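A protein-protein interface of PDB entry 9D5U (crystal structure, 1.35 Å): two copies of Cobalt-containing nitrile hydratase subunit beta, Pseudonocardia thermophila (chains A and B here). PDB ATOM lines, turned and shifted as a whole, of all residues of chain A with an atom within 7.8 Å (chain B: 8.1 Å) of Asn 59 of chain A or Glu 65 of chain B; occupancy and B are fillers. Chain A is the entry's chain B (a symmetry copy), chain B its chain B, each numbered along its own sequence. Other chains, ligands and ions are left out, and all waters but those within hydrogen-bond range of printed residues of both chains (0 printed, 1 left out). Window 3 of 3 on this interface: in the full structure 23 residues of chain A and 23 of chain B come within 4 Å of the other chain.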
ATOM      1  N   VAL A   4      -2.884  -1.036  10.802  1.00  0.00           N
ATOM      2  CA  VAL A   4      -1.486  -0.630  10.975  1.00  0.00           C
ATOM      3  C   VAL A   4      -0.995   0.187   9.789  1.00  0.00           C
ATOM      4  O   VAL A   4      -0.076   1.005   9.928  1.00  0.00           O
ATOM      5  CB  VAL A   4      -0.570  -1.844  11.270  1.00  0.00           C
ATOM      6  CG1 VAL A   4       0.890  -1.419  11.267  1.00  0.00           C
ATOM      7  CG2 VAL A   4      -0.920  -2.478  12.616  1.00  0.00           C
ATOM      8  N   GLY A  54      -8.468  -4.007   0.454  1.00  0.00           N
ATOM      9  CA  GLY A  54      -7.898  -5.351   0.548  1.00  0.00           C
ATOM     10  C   GLY A  54      -6.513  -5.331   1.169  1.00  0.00           C
ATOM     11  O   GLY A  54      -6.192  -6.146   2.039  1.00  0.00           O
ATOM     12  N   ILE A  55      -5.676  -4.379   0.746  1.00  0.00           N
ATOM     13  CA  ILE A  55      -4.356  -4.238   1.343  1.00  0.00           C
ATOM     14  C   ILE A  55      -4.471  -3.897   2.830  1.00  0.00           C
ATOM     15  O   ILE A  55      -3.681  -4.380   3.655  1.00  0.00           O
ATOM     16  CB  ILE A  55      -3.540  -3.193   0.552  1.00  0.00           C
ATOM     17  CG1 ILE A  55      -3.313  -3.670  -0.894  1.00  0.00           C
ATOM     18  CG2 ILE A  55      -2.224  -2.866   1.281  1.00  0.00           C
ATOM     19  CD1 ILE A  55      -2.561  -2.667  -1.810  1.00  0.00           C
ATOM     20  N   GLU A  56      -5.467  -3.077   3.205  1.00  0.00           N
ATOM     21  CA  GLU A  56      -5.634  -2.654   4.600  1.00  0.00           C
ATOM     22  C   GLU A  56      -6.054  -3.791   5.537  1.00  0.00           C
ATOM     23  O   GLU A  56      -5.972  -3.626   6.764  1.00  0.00           O
ATOM     24  CB  GLU A  56      -6.650  -1.513   4.676  1.00  0.00           C
ATOM     25  CG  GLU A  56      -6.221  -0.264   3.907  1.00  0.00           C
ATOM     26  CD  GLU A  56      -7.354   0.713   3.641  1.00  0.00           C
ATOM     27  OE1 GLU A  56      -8.504   0.440   3.994  1.00  0.00           O
ATOM     28  OE2 GLU A  56      -7.088   1.773   3.070  1.00  0.00           O
ATOM     29  N   GLN A  57      -6.503  -4.932   5.002  1.00  0.00           N
ATOM     30  CA  GLN A  57      -6.908  -6.084   5.814  1.00  0.00           C
ATOM     31  C   GLN A  57      -5.824  -7.156   5.891  1.00  0.00           C
ATOM     32  O   GLN A  57      -6.065  -8.262   6.409  1.00  0.00           O
ATOM     33  CB  GLN A  57      -8.201  -6.667   5.258  1.00  0.00           C
ATOM     34  CG  GLN A  57      -9.383  -5.708   5.312  1.00  0.00           C
ATOM     35  CD  GLN A  57     -10.574  -6.240   4.561  1.00  0.00           C
ATOM     36  OE1 GLN A  57     -11.278  -7.116   5.051  1.00  0.00           O
ATOM     37  NE2 GLN A  57     -10.806  -5.722   3.348  1.00  0.00           N
ATOM     38  N   MET A  58      -4.640  -6.845   5.369  1.00  0.00           N
ATOM     39  CA  MET A  58      -3.482  -7.713   5.411  1.00  0.00           C
ATOM     40  C   MET A  58      -3.072  -7.963   6.863  1.00  0.00           C
ATOM     41  O   MET A  58      -3.396  -7.196   7.782  1.00  0.00           O
ATOM     42  CB  MET A  58      -2.356  -6.987   4.657  1.00  0.00           C
ATOM     43  CG  MET A  58      -2.203  -7.423   3.196  1.00  0.00           C
ATOM     44  SD  MET A  58      -0.762  -6.649   2.419  1.00  0.00           S
ATOM     45  CE  MET A  58       0.564  -7.677   3.127  1.00  0.00           C
ATOM     46  N   ASN A  59      -2.349  -9.057   7.072  1.00  0.00           N
ATOM     47  CA  ASN A  59      -1.700  -9.252   8.349  1.00  0.00           C
ATOM     48  C   ASN A  59      -0.694  -8.113   8.556  1.00  0.00           C
ATOM     49  O   ASN A  59       0.061  -7.773   7.621  1.00  0.00           O
ATOM     50  CB  ASN A  59      -1.035 -10.632   8.349  1.00  0.00           C
ATOM     51  CG  ASN A  59       0.004 -10.804   9.449  1.00  0.00           C
ATOM     52  OD1 ASN A  59       0.520  -9.843  10.030  1.00  0.00           O
ATOM     53  ND2 ASN A  59       0.270 -12.062   9.789  1.00  0.00           N
ATOM     54  N   PRO A  60      -0.679  -7.470   9.727  1.00  0.00           N
ATOM     55  CA  PRO A  60       0.122  -6.243   9.870  1.00  0.00           C
ATOM     56  C   PRO A  60       1.628  -6.463   9.777  1.00  0.00           C
ATOM     57  O   PRO A  60       2.321  -5.628   9.168  1.00  0.00           O
ATOM     58  CB  PRO A  60      -0.305  -5.727  11.257  1.00  0.00           C
ATOM     59  CG  PRO A  60      -1.670  -6.228  11.412  1.00  0.00           C
ATOM     60  CD  PRO A  60      -1.586  -7.639  10.872  1.00  0.00           C
ATOM     61  N   ALA A  61       2.163  -7.551  10.369  1.00  0.00           N
ATOM     62  CA  ALA A  61       3.614  -7.783  10.321  1.00  0.00           C
ATOM     63  C   ALA A  61       4.087  -8.055   8.898  1.00  0.00           C
ATOM     64  O   ALA A  61       5.141  -7.560   8.482  1.00  0.00           O
ATOM     65  CB  ALA A  61       4.010  -8.939  11.248  1.00  0.00           C
ATOM     66  N   GLU A  62       3.311  -8.828   8.142  1.00  0.00           N
ATOM     67  CA  GLU A  62       3.588  -9.047   6.731  1.00  0.00           C
ATOM     68  C   GLU A  62       3.495  -7.751   5.920  1.00  0.00           C
ATOM     69  O   GLU A  62       4.380  -7.455   5.114  1.00  0.00           O
ATOM     70  CB  GLU A  62       2.592 -10.066   6.183  1.00  0.00           C
ATOM     71  CG  GLU A  62       2.951 -10.559   4.832  1.00  0.00           C
ATOM     72  CD  GLU A  62       1.891 -11.429   4.278  1.00  0.00           C
ATOM     73  OE1 GLU A  62       0.930 -10.899   3.691  1.00  0.00           O
ATOM     74  OE2 GLU A  62       2.007 -12.661   4.438  1.00  0.00           O
ATOM     75  N   TYR A  63       2.402  -6.992   6.070  1.00  0.00           N
ATOM     76  CA  TYR A  63       2.291  -5.711   5.384  1.00  0.00           C
ATOM     77  C   TYR A  63       3.554  -4.879   5.574  1.00  0.00           C
ATOM     78  O   TYR A  63       4.104  -4.330   4.609  1.00  0.00           O
ATOM     79  CB  TYR A  63       1.082  -4.947   5.920  1.00  0.00           C
ATOM     80  CG  TYR A  63       1.032  -3.509   5.434  1.00  0.00           C
ATOM     81  CD1 TYR A  63       0.504  -3.203   4.205  1.00  0.00           C
ATOM     82  CD2 TYR A  63       1.551  -2.470   6.208  1.00  0.00           C
ATOM     83  CE1 TYR A  63       0.460  -1.930   3.753  1.00  0.00           C
ATOM     84  CE2 TYR A  63       1.518  -1.179   5.762  1.00  0.00           C
ATOM     85  CZ  TYR A  63       0.972  -0.922   4.544  1.00  0.00           C
ATOM     86  OH  TYR A  63       0.894   0.368   4.068  1.00  0.00           O
ATOM     87  N   LEU A  64       4.039  -4.801   6.824  1.00  0.00           N
ATOM     88  CA  LEU A  64       5.121  -3.889   7.202  1.00  0.00           C
ATOM     89  C   LEU A  64       6.462  -4.279   6.589  1.00  0.00           C
ATOM     90  O   LEU A  64       7.297  -3.395   6.327  1.00  0.00           O
ATOM     91  CB  LEU A  64       5.274  -3.881   8.721  1.00  0.00           C
ATOM     92  CG  LEU A  64       4.160  -3.247   9.547  1.00  0.00           C
ATOM     93  CD1 LEU A  64       4.408  -3.562  11.010  1.00  0.00           C
ATOM     94  CD2 LEU A  64       4.090  -1.758   9.313  1.00  0.00           C
ATOM     95  N   GLU A  65       6.708  -5.581   6.394  1.00  0.00           N
ATOM     96  CA  GLU A  65       7.999  -6.081   5.924  1.00  0.00           C
ATOM     97  C   GLU A  65       7.969  -6.867   4.606  1.00  0.00           C
ATOM     98  O   GLU A  65       9.014  -7.339   4.164  1.00  0.00           O
ATOM     99  CB  GLU A  65       8.702  -6.918   7.003  1.00  0.00           C
ATOM    100  CG  GLU A  65       9.046  -6.160   8.280  1.00  0.00           C
ATOM    101  CD  GLU A  65       9.984  -6.967   9.223  1.00  0.00           C
ATOM    102  OE1 GLU A  65       9.878  -8.204   9.298  1.00  0.00           O
ATOM    103  OE2 GLU A  65      10.826  -6.364   9.895  1.00  0.00           O
ATOM    104  N   SER A  66       6.843  -7.019   3.967  1.00  0.00           N
ATOM    105  CA  SER A  66       6.856  -7.721   2.705  1.00  0.00           C
ATOM    106  C   SER A  66       7.213  -6.761   1.565  1.00  0.00           C
ATOM    107  O   SER A  66       7.078  -5.537   1.701  1.00  0.00           O
ATOM    108  CB  SER A  66       5.477  -8.317   2.434  1.00  0.00           C
ATOM    109  OG  SER A  66       4.500  -7.284   2.299  1.00  0.00           O
ATOM    110  N   HIS A  71       1.762  -6.831  -1.498  1.00  0.00           N
ATOM    111  CA  HIS A  71       0.471  -6.277  -1.075  1.00  0.00           C
ATOM    112  C   HIS A  71      -0.564  -6.397  -2.187  1.00  0.00           C
ATOM    113  O   HIS A  71      -1.718  -6.793  -1.944  1.00  0.00           O
ATOM    114  CB  HIS A  71       0.628  -4.810  -0.694  1.00  0.00           C
ATOM    115  CG  HIS A  71       1.690  -4.567   0.329  1.00  0.00           C
ATOM    116  ND1 HIS A  71       1.984  -3.306   0.808  1.00  0.00           N
ATOM    117  CD2 HIS A  71       2.548  -5.413   0.949  1.00  0.00           C
ATOM    118  CE1 HIS A  71       2.964  -3.393   1.690  1.00  0.00           C
ATOM    119  NE2 HIS A  71       3.330  -4.659   1.786  1.00  0.00           N
ATOM    120  N   ARG A  74      -1.953  -9.879  -2.503  1.00  0.00           N
ATOM    121  CA  ARG A  74      -2.911 -10.156  -1.434  1.00  0.00           C
ATOM    122  C   ARG A  74      -4.283  -9.575  -1.743  1.00  0.00           C
ATOM    123  O   ARG A  74      -5.315 -10.262  -1.620  1.00  0.00           O
ATOM    124  CB  ARG A  74      -2.389  -9.591  -0.130  1.00  0.00           C
ATOM    125  CG  ARG A  74      -1.325 -10.469   0.503  1.00  0.00           C
ATOM    126  CD  ARG A  74      -1.874 -11.837   0.878  1.00  0.00           C
ATOM    127  NE  ARG A  74      -0.975 -12.512   1.805  1.00  0.00           N
ATOM    128  CZ  ARG A  74      -1.066 -13.797   2.121  1.00  0.00           C
ATOM    129  NH1 ARG A  74      -2.028 -14.559   1.626  1.00  0.00           N
ATOM    130  NH2 ARG A  74      -0.187 -14.320   2.974  1.00  0.00           N
ATOM    131  N   GLY B  12      -7.749  -4.952  12.691  1.00  0.00           N
ATOM    132  CA  GLY B  12      -7.109  -5.841  11.739  1.00  0.00           C
ATOM    133  C   GLY B  12      -5.977  -6.667  12.287  1.00  0.00           C
ATOM    134  O   GLY B  12      -5.165  -7.166  11.493  1.00  0.00           O
ATOM    135  N   LEU B  13      -5.887  -6.817  13.620  1.00  0.00           N
ATOM    136  CA  LEU B  13      -4.848  -7.640  14.238  1.00  0.00           C
ATOM    137  C   LEU B  13      -5.187  -9.140  14.263  1.00  0.00           C
ATOM    138  O   LEU B  13      -4.286  -9.967  14.489  1.00  0.00           O
ATOM    139  CB  LEU B  13      -4.492  -7.129  15.642  1.00  0.00           C
ATOM    140  CG  LEU B  13      -4.059  -5.659  15.680  1.00  0.00           C
ATOM    141  CD1 LEU B  13      -3.350  -5.266  16.987  1.00  0.00           C
ATOM    142  CD2 LEU B  13      -3.177  -5.329  14.476  1.00  0.00           C
ATOM    143  N   GLY B  14      -6.454  -9.501  14.031  1.00  0.00           N
ATOM    144  CA  GLY B  14      -6.853 -10.879  13.888  1.00  0.00           C
ATOM    145  C   GLY B  14      -7.504 -11.426  15.134  1.00  0.00           C
ATOM    146  O   GLY B  14      -7.520 -10.792  16.190  1.00  0.00           O
ATOM    147  N   MET B  58      11.356  -2.000  20.124  1.00  0.00           N
ATOM    148  CA  MET B  58      11.511  -3.208  19.340  1.00  0.00           C
ATOM    149  C   MET B  58      11.093  -2.943  17.893  1.00  0.00           C
ATOM    150  O   MET B  58      10.339  -2.010  17.583  1.00  0.00           O
ATOM    151  CB  MET B  58      10.598  -4.269  19.974  1.00  0.00           C
ATOM    152  CG  MET B  58      11.319  -5.214  20.940  1.00  0.00           C
ATOM    153  SD  MET B  58      10.224  -6.533  21.522  1.00  0.00           S
ATOM    154  CE  MET B  58      10.234  -7.616  20.057  1.00  0.00           C
ATOM    155  N   ASN B  59      11.593  -3.781  16.992  1.00  0.00           N
ATOM    156  CA  ASN B  59      11.067  -3.781  15.645  1.00  0.00           C
ATOM    157  C   ASN B  59       9.584  -4.167  15.708  1.00  0.00           C
ATOM    158  O   ASN B  59       9.220  -5.124  16.421  1.00  0.00           O
ATOM    159  CB  ASN B  59      11.894  -4.756  14.801  1.00  0.00           C
ATOM    160  CG  ASN B  59      11.215  -5.155  13.498  1.00  0.00           C
ATOM    161  OD1 ASN B  59      10.002  -5.014  13.311  1.00  0.00           O
ATOM    162  ND2 ASN B  59      12.031  -5.603  12.547  1.00  0.00           N
ATOM    163  N   PRO B  60       8.697  -3.431  15.030  1.00  0.00           N
ATOM    164  CA  PRO B  60       7.257  -3.650  15.248  1.00  0.00           C
ATOM    165  C   PRO B  60       6.751  -5.010  14.776  1.00  0.00           C
ATOM    166  O   PRO B  60       5.910  -5.612  15.468  1.00  0.00           O
ATOM    167  CB  PRO B  60       6.621  -2.489  14.462  1.00  0.00           C
ATOM    168  CG  PRO B  60       7.639  -1.440  14.503  1.00  0.00           C
ATOM    169  CD  PRO B  60       8.928  -2.197  14.267  1.00  0.00           C
ATOM    170  N   ALA B  61       7.222  -5.511  13.614  1.00  0.00           N
ATOM    171  CA  ALA B  61       6.739  -6.805  13.116  1.00  0.00           C
ATOM    172  C   ALA B  61       7.160  -7.948  14.033  1.00  0.00           C
ATOM    173  O   ALA B  61       6.373  -8.863  14.298  1.00  0.00           O
ATOM    174  CB  ALA B  61       7.232  -7.055  11.686  1.00  0.00           C
ATOM    175  N   GLU B  62       8.394  -7.897  14.530  1.00  0.00           N
ATOM    176  CA  GLU B  62       8.861  -8.855  15.519  1.00  0.00           C
ATOM    177  C   GLU B  62       8.073  -8.758  16.829  1.00  0.00           C
ATOM    178  O   GLU B  62       7.646  -9.778  17.377  1.00  0.00           O
ATOM    179  CB  GLU B  62      10.342  -8.601  15.794  1.00  0.00           C
ATOM    180  CG  GLU B  62      10.980  -9.682  16.581  1.00  0.00           C
ATOM    181  CD  GLU B  62      12.370  -9.331  16.948  1.00  0.00           C
ATOM    182  OE1 GLU B  62      12.561  -8.647  17.971  1.00  0.00           O
ATOM    183  OE2 GLU B  62      13.286  -9.732  16.205  1.00  0.00           O
ATOM    184  N   TYR B  63       7.920  -7.549  17.384  1.00  0.00           N
ATOM    185  CA  TYR B  63       7.116  -7.384  18.588  1.00  0.00           C
ATOM    186  C   TYR B  63       5.769  -8.085  18.445  1.00  0.00           C
ATOM    187  O   TYR B  63       5.339  -8.823  19.342  1.00  0.00           O
ATOM    188  CB  TYR B  63       6.898  -5.896  18.858  1.00  0.00           C
ATOM    189  CG  TYR B  63       5.876  -5.640  19.950  1.00  0.00           C
ATOM    190  CD1 TYR B  63       6.238  -5.684  21.274  1.00  0.00           C
ATOM    191  CD2 TYR B  63       4.539  -5.387  19.639  1.00  0.00           C
ATOM    192  CE1 TYR B  63       5.338  -5.468  22.259  1.00  0.00           C
ATOM    193  CE2 TYR B  63       3.618  -5.171  20.625  1.00  0.00           C
ATOM    194  CZ  TYR B  63       4.026  -5.211  21.921  1.00  0.00           C
ATOM    195  OH  TYR B  63       3.135  -4.972  22.945  1.00  0.00           O
ATOM    196  N   LEU B  64       5.104  -7.877  17.297  1.00  0.00           N
ATOM    197  CA  LEU B  64       3.722  -8.315  17.089  1.00  0.00           C
ATOM    198  C   LEU B  64       3.588  -9.833  17.019  1.00  0.00           C
ATOM    199  O   LEU B  64       2.537 -10.375  17.403  1.00  0.00           O
ATOM    200  CB  LEU B  64       3.192  -7.728  15.783  1.00  0.00           C
ATOM    201  CG  LEU B  64       2.951  -6.223  15.723  1.00  0.00           C
ATOM    202  CD1 LEU B  64       2.660  -5.841  14.284  1.00  0.00           C
ATOM    203  CD2 LEU B  64       1.821  -5.817  16.635  1.00  0.00           C
ATOM    204  N   GLU B  65       4.608 -10.529  16.498  1.00  0.00           N
ATOM    205  CA  GLU B  65       4.547 -11.973  16.273  1.00  0.00           C
ATOM    206  C   GLU B  65       5.604 -12.806  17.010  1.00  0.00           C
ATOM    207  O   GLU B  65       5.627 -14.025  16.847  1.00  0.00           O
ATOM    208  CB  GLU B  65       4.585 -12.308  14.774  1.00  0.00           C
ATOM    209  CG  GLU B  65       3.415 -11.760  13.964  1.00  0.00           C
ATOM    210  CD  GLU B  65       3.359 -12.344  12.522  1.00  0.00           C
ATOM    211  OE1 GLU B  65       4.411 -12.602  11.913  1.00  0.00           O
ATOM    212  OE2 GLU B  65       2.260 -12.541  11.996  1.00  0.00           O
ATOM    213  N   SER B  66       6.454 -12.221  17.805  1.00  0.00           N
ATOM    214  CA  SER B  66       7.404 -13.039  18.522  1.00  0.00           C
ATOM    215  C   SER B  66       6.777 -13.572  19.815  1.00  0.00           C
ATOM    216  O   SER B  66       5.787 -13.020  20.315  1.00  0.00           O
ATOM    217  CB  SER B  66       8.634 -12.207  18.877  1.00  0.00           C
ATOM    218  OG  SER B  66       8.282 -11.143  19.764  1.00  0.00           O
ATOM    219  N   PRO B  67       7.360 -14.631  20.399  1.00  0.00           N
ATOM    220  CA  PRO B  67       6.963 -15.043  21.750  1.00  0.00           C
ATOM    221  C   PRO B  67       7.144 -13.908  22.749  1.00  0.00           C
ATOM    222  O   PRO B  67       8.152 -13.210  22.746  1.00  0.00           O
ATOM    223  CB  PRO B  67       7.927 -16.200  22.049  1.00  0.00           C
ATOM    224  CG  PRO B  67       8.212 -16.786  20.677  1.00  0.00           C
ATOM    225  CD  PRO B  67       8.375 -15.553  19.832  1.00  0.00           C
ATOM    226  N   TYR B  68       6.158 -13.756  23.633  1.00  0.00           N
ATOM    227  CA  TYR B  68       6.152 -12.678  24.617  1.00  0.00           C
ATOM    228  C   TYR B  68       7.502 -12.498  25.300  1.00  0.00           C
ATOM    229  O   TYR B  68       8.044 -11.390  25.328  1.00  0.00           O
ATOM    230  CB  TYR B  68       5.054 -12.930  25.658  1.00  0.00           C
ATOM    231  CG  TYR B  68       5.042 -11.911  26.760  1.00  0.00           C
ATOM    232  CD1 TYR B  68       4.458 -10.656  26.569  1.00  0.00           C
ATOM    233  CD2 TYR B  68       5.654 -12.179  27.987  1.00  0.00           C
ATOM    234  CE1 TYR B  68       4.450  -9.698  27.583  1.00  0.00           C
ATOM    235  CE2 TYR B  68       5.660 -11.232  29.001  1.00  0.00           C
ATOM    236  CZ  TYR B  68       5.045  -9.979  28.782  1.00  0.00           C
ATOM    237  OH  TYR B  68       5.034  -9.042  29.777  1.00  0.00           O
ATOM    238  N   TRP B  70      10.410 -13.261  24.564  1.00  0.00           N
ATOM    239  CA  TRP B  70      11.422 -12.713  23.666  1.00  0.00           C
ATOM    240  C   TRP B  70      11.490 -11.182  23.763  1.00  0.00           C
ATOM    241  O   TRP B  70      12.581 -10.593  23.662  1.00  0.00           O
ATOM    242  CB  TRP B  70      11.158 -13.141  22.227  1.00  0.00           C
ATOM    243  CG  TRP B  70      12.129 -12.473  21.355  1.00  0.00           C
ATOM    244  CD1 TRP B  70      11.889 -11.508  20.441  1.00  0.00           C
ATOM    245  CD2 TRP B  70      13.540 -12.663  21.392  1.00  0.00           C
ATOM    246  NE1 TRP B  70      13.072 -11.111  19.852  1.00  0.00           N
ATOM    247  CE2 TRP B  70      14.101 -11.801  20.431  1.00  0.00           C
ATOM    248  CE3 TRP B  70      14.390 -13.499  22.142  1.00  0.00           C
ATOM    249  CZ2 TRP B  70      15.475 -11.745  20.196  1.00  0.00           C
ATOM    250  CZ3 TRP B  70      15.758 -13.440  21.919  1.00  0.00           C
ATOM    251  CH2 TRP B  70      16.289 -12.572  20.957  1.00  0.00           C
ATOM    252  N   HIS B  71      10.336 -10.515  23.948  1.00  0.00           N
ATOM    253  CA  HIS B  71      10.365  -9.077  24.238  1.00  0.00           C
ATOM    254  C   HIS B  71      11.287  -8.777  25.414  1.00  0.00           C
ATOM    255  O   HIS B  71      12.091  -7.830  25.369  1.00  0.00           O
ATOM    256  CB  HIS B  71       8.963  -8.576  24.561  1.00  0.00           C
ATOM    257  CG  HIS B  71       7.953  -8.901  23.509  1.00  0.00           C
ATOM    258  ND1 HIS B  71       6.626  -8.533  23.614  1.00  0.00           N
ATOM    259  CD2 HIS B  71       8.061  -9.583  22.342  1.00  0.00           C
ATOM    260  CE1 HIS B  71       5.971  -8.957  22.548  1.00  0.00           C
ATOM    261  NE2 HIS B  71       6.817  -9.606  21.767  1.00  0.00           N
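Of the 16 printed residues of chain B, 5 touch a printed residue of chain A.
Hydrophobic or aromatic side chains of chain B within 4 Å of the printed part of chain A: Leu 13 and Ala 61.
Among the printed residues, 7 pairs touch across the chains.
Among the printed residues, no Asp or Glu carboxylate lies within 4 Å of a Lys or Arg side-chain nitrogen of the other chain.
Asn 59 of chain A touches just one residue of chain B: Glu 65 (3.0 Å).
Of chain A, only Asn 59 and Ala 61 come within 4 Å of Glu 65 of chain B.
Pro 60 of chain A touches just these residues of chain B: Gly 12 and Leu 13.
Printed residues of chain B within 4 Å of Glu 65 of chain A: Asn 59 (3.0 Å) and Ala 61 (3.7 Å).
Of the printed residues of chain A, Ala 61 of chain B touches Ala 61 and Glu 65.
Printed residues of chain A within 4 Å of Asn 59 of chain B: Glu 65.
Of the printed residues of chain B, Ala 61 of chain A touches Ala 61 and Glu 65.
Ile 55 of chain A touches none of the printed residues of chain B.
Pro 67 of chain B touches none of the printed residues of chain A.
The nearest residue of chain B that does not touch Asn 59 of chain A is Gly 12 of chain B (5.1 Å).
The side-chain amide nitrogen (ND2) of Asn 59 of chain B sits at hydrogen-bond distance from the side-chain carboxylate (OE2) of Glu 65 of chain A, 3.0 Å away.
ND2 of Asn 59 of chain A sits at hydrogen-bond distance from OE2 of Glu 65 of chain B, 3.0 Å away.
Asn 59 of chain A touches Glu 65 of chain B, and with the chains exchanged Glu 65 of chain A touches Asn 59 of chain B.
Ala 61 of chain A touches its own counterpart, Ala 61 of chain B.
Ala 61 of chain A touches Glu 65 of chain B, and with the chains exchanged Glu 65 of chain A touches Ala 61 of chain B.
Of the 7 pairs that touch across the chains among the printed residues, 5 have their exchanged pair printed and touching as well.
N of Ala 61 of chain B lies within hydrogen-bond range of OD1 of Asn 59 of chain B, at 2.8 Å.
N of Ala 61 of chain A lies within hydrogen-bond range of OD1 of Asn 59 of chain A (2.8 Å).
Among the printed residues, pairs that only touch across the chains: Pro 60 of chain A with Leu 13 of chain B (3.5 Å), Pro 60 of chain A with Gly 12 of chain B (3.6 Å), Ala 61 of chain A with Glu 65 of chain B (3.7 Å), Glu 65 of chain A with Ala 61 of chain B (3.7 Å) and Ala 61 of chain A with Ala 61 of chain B (3.8 Å).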
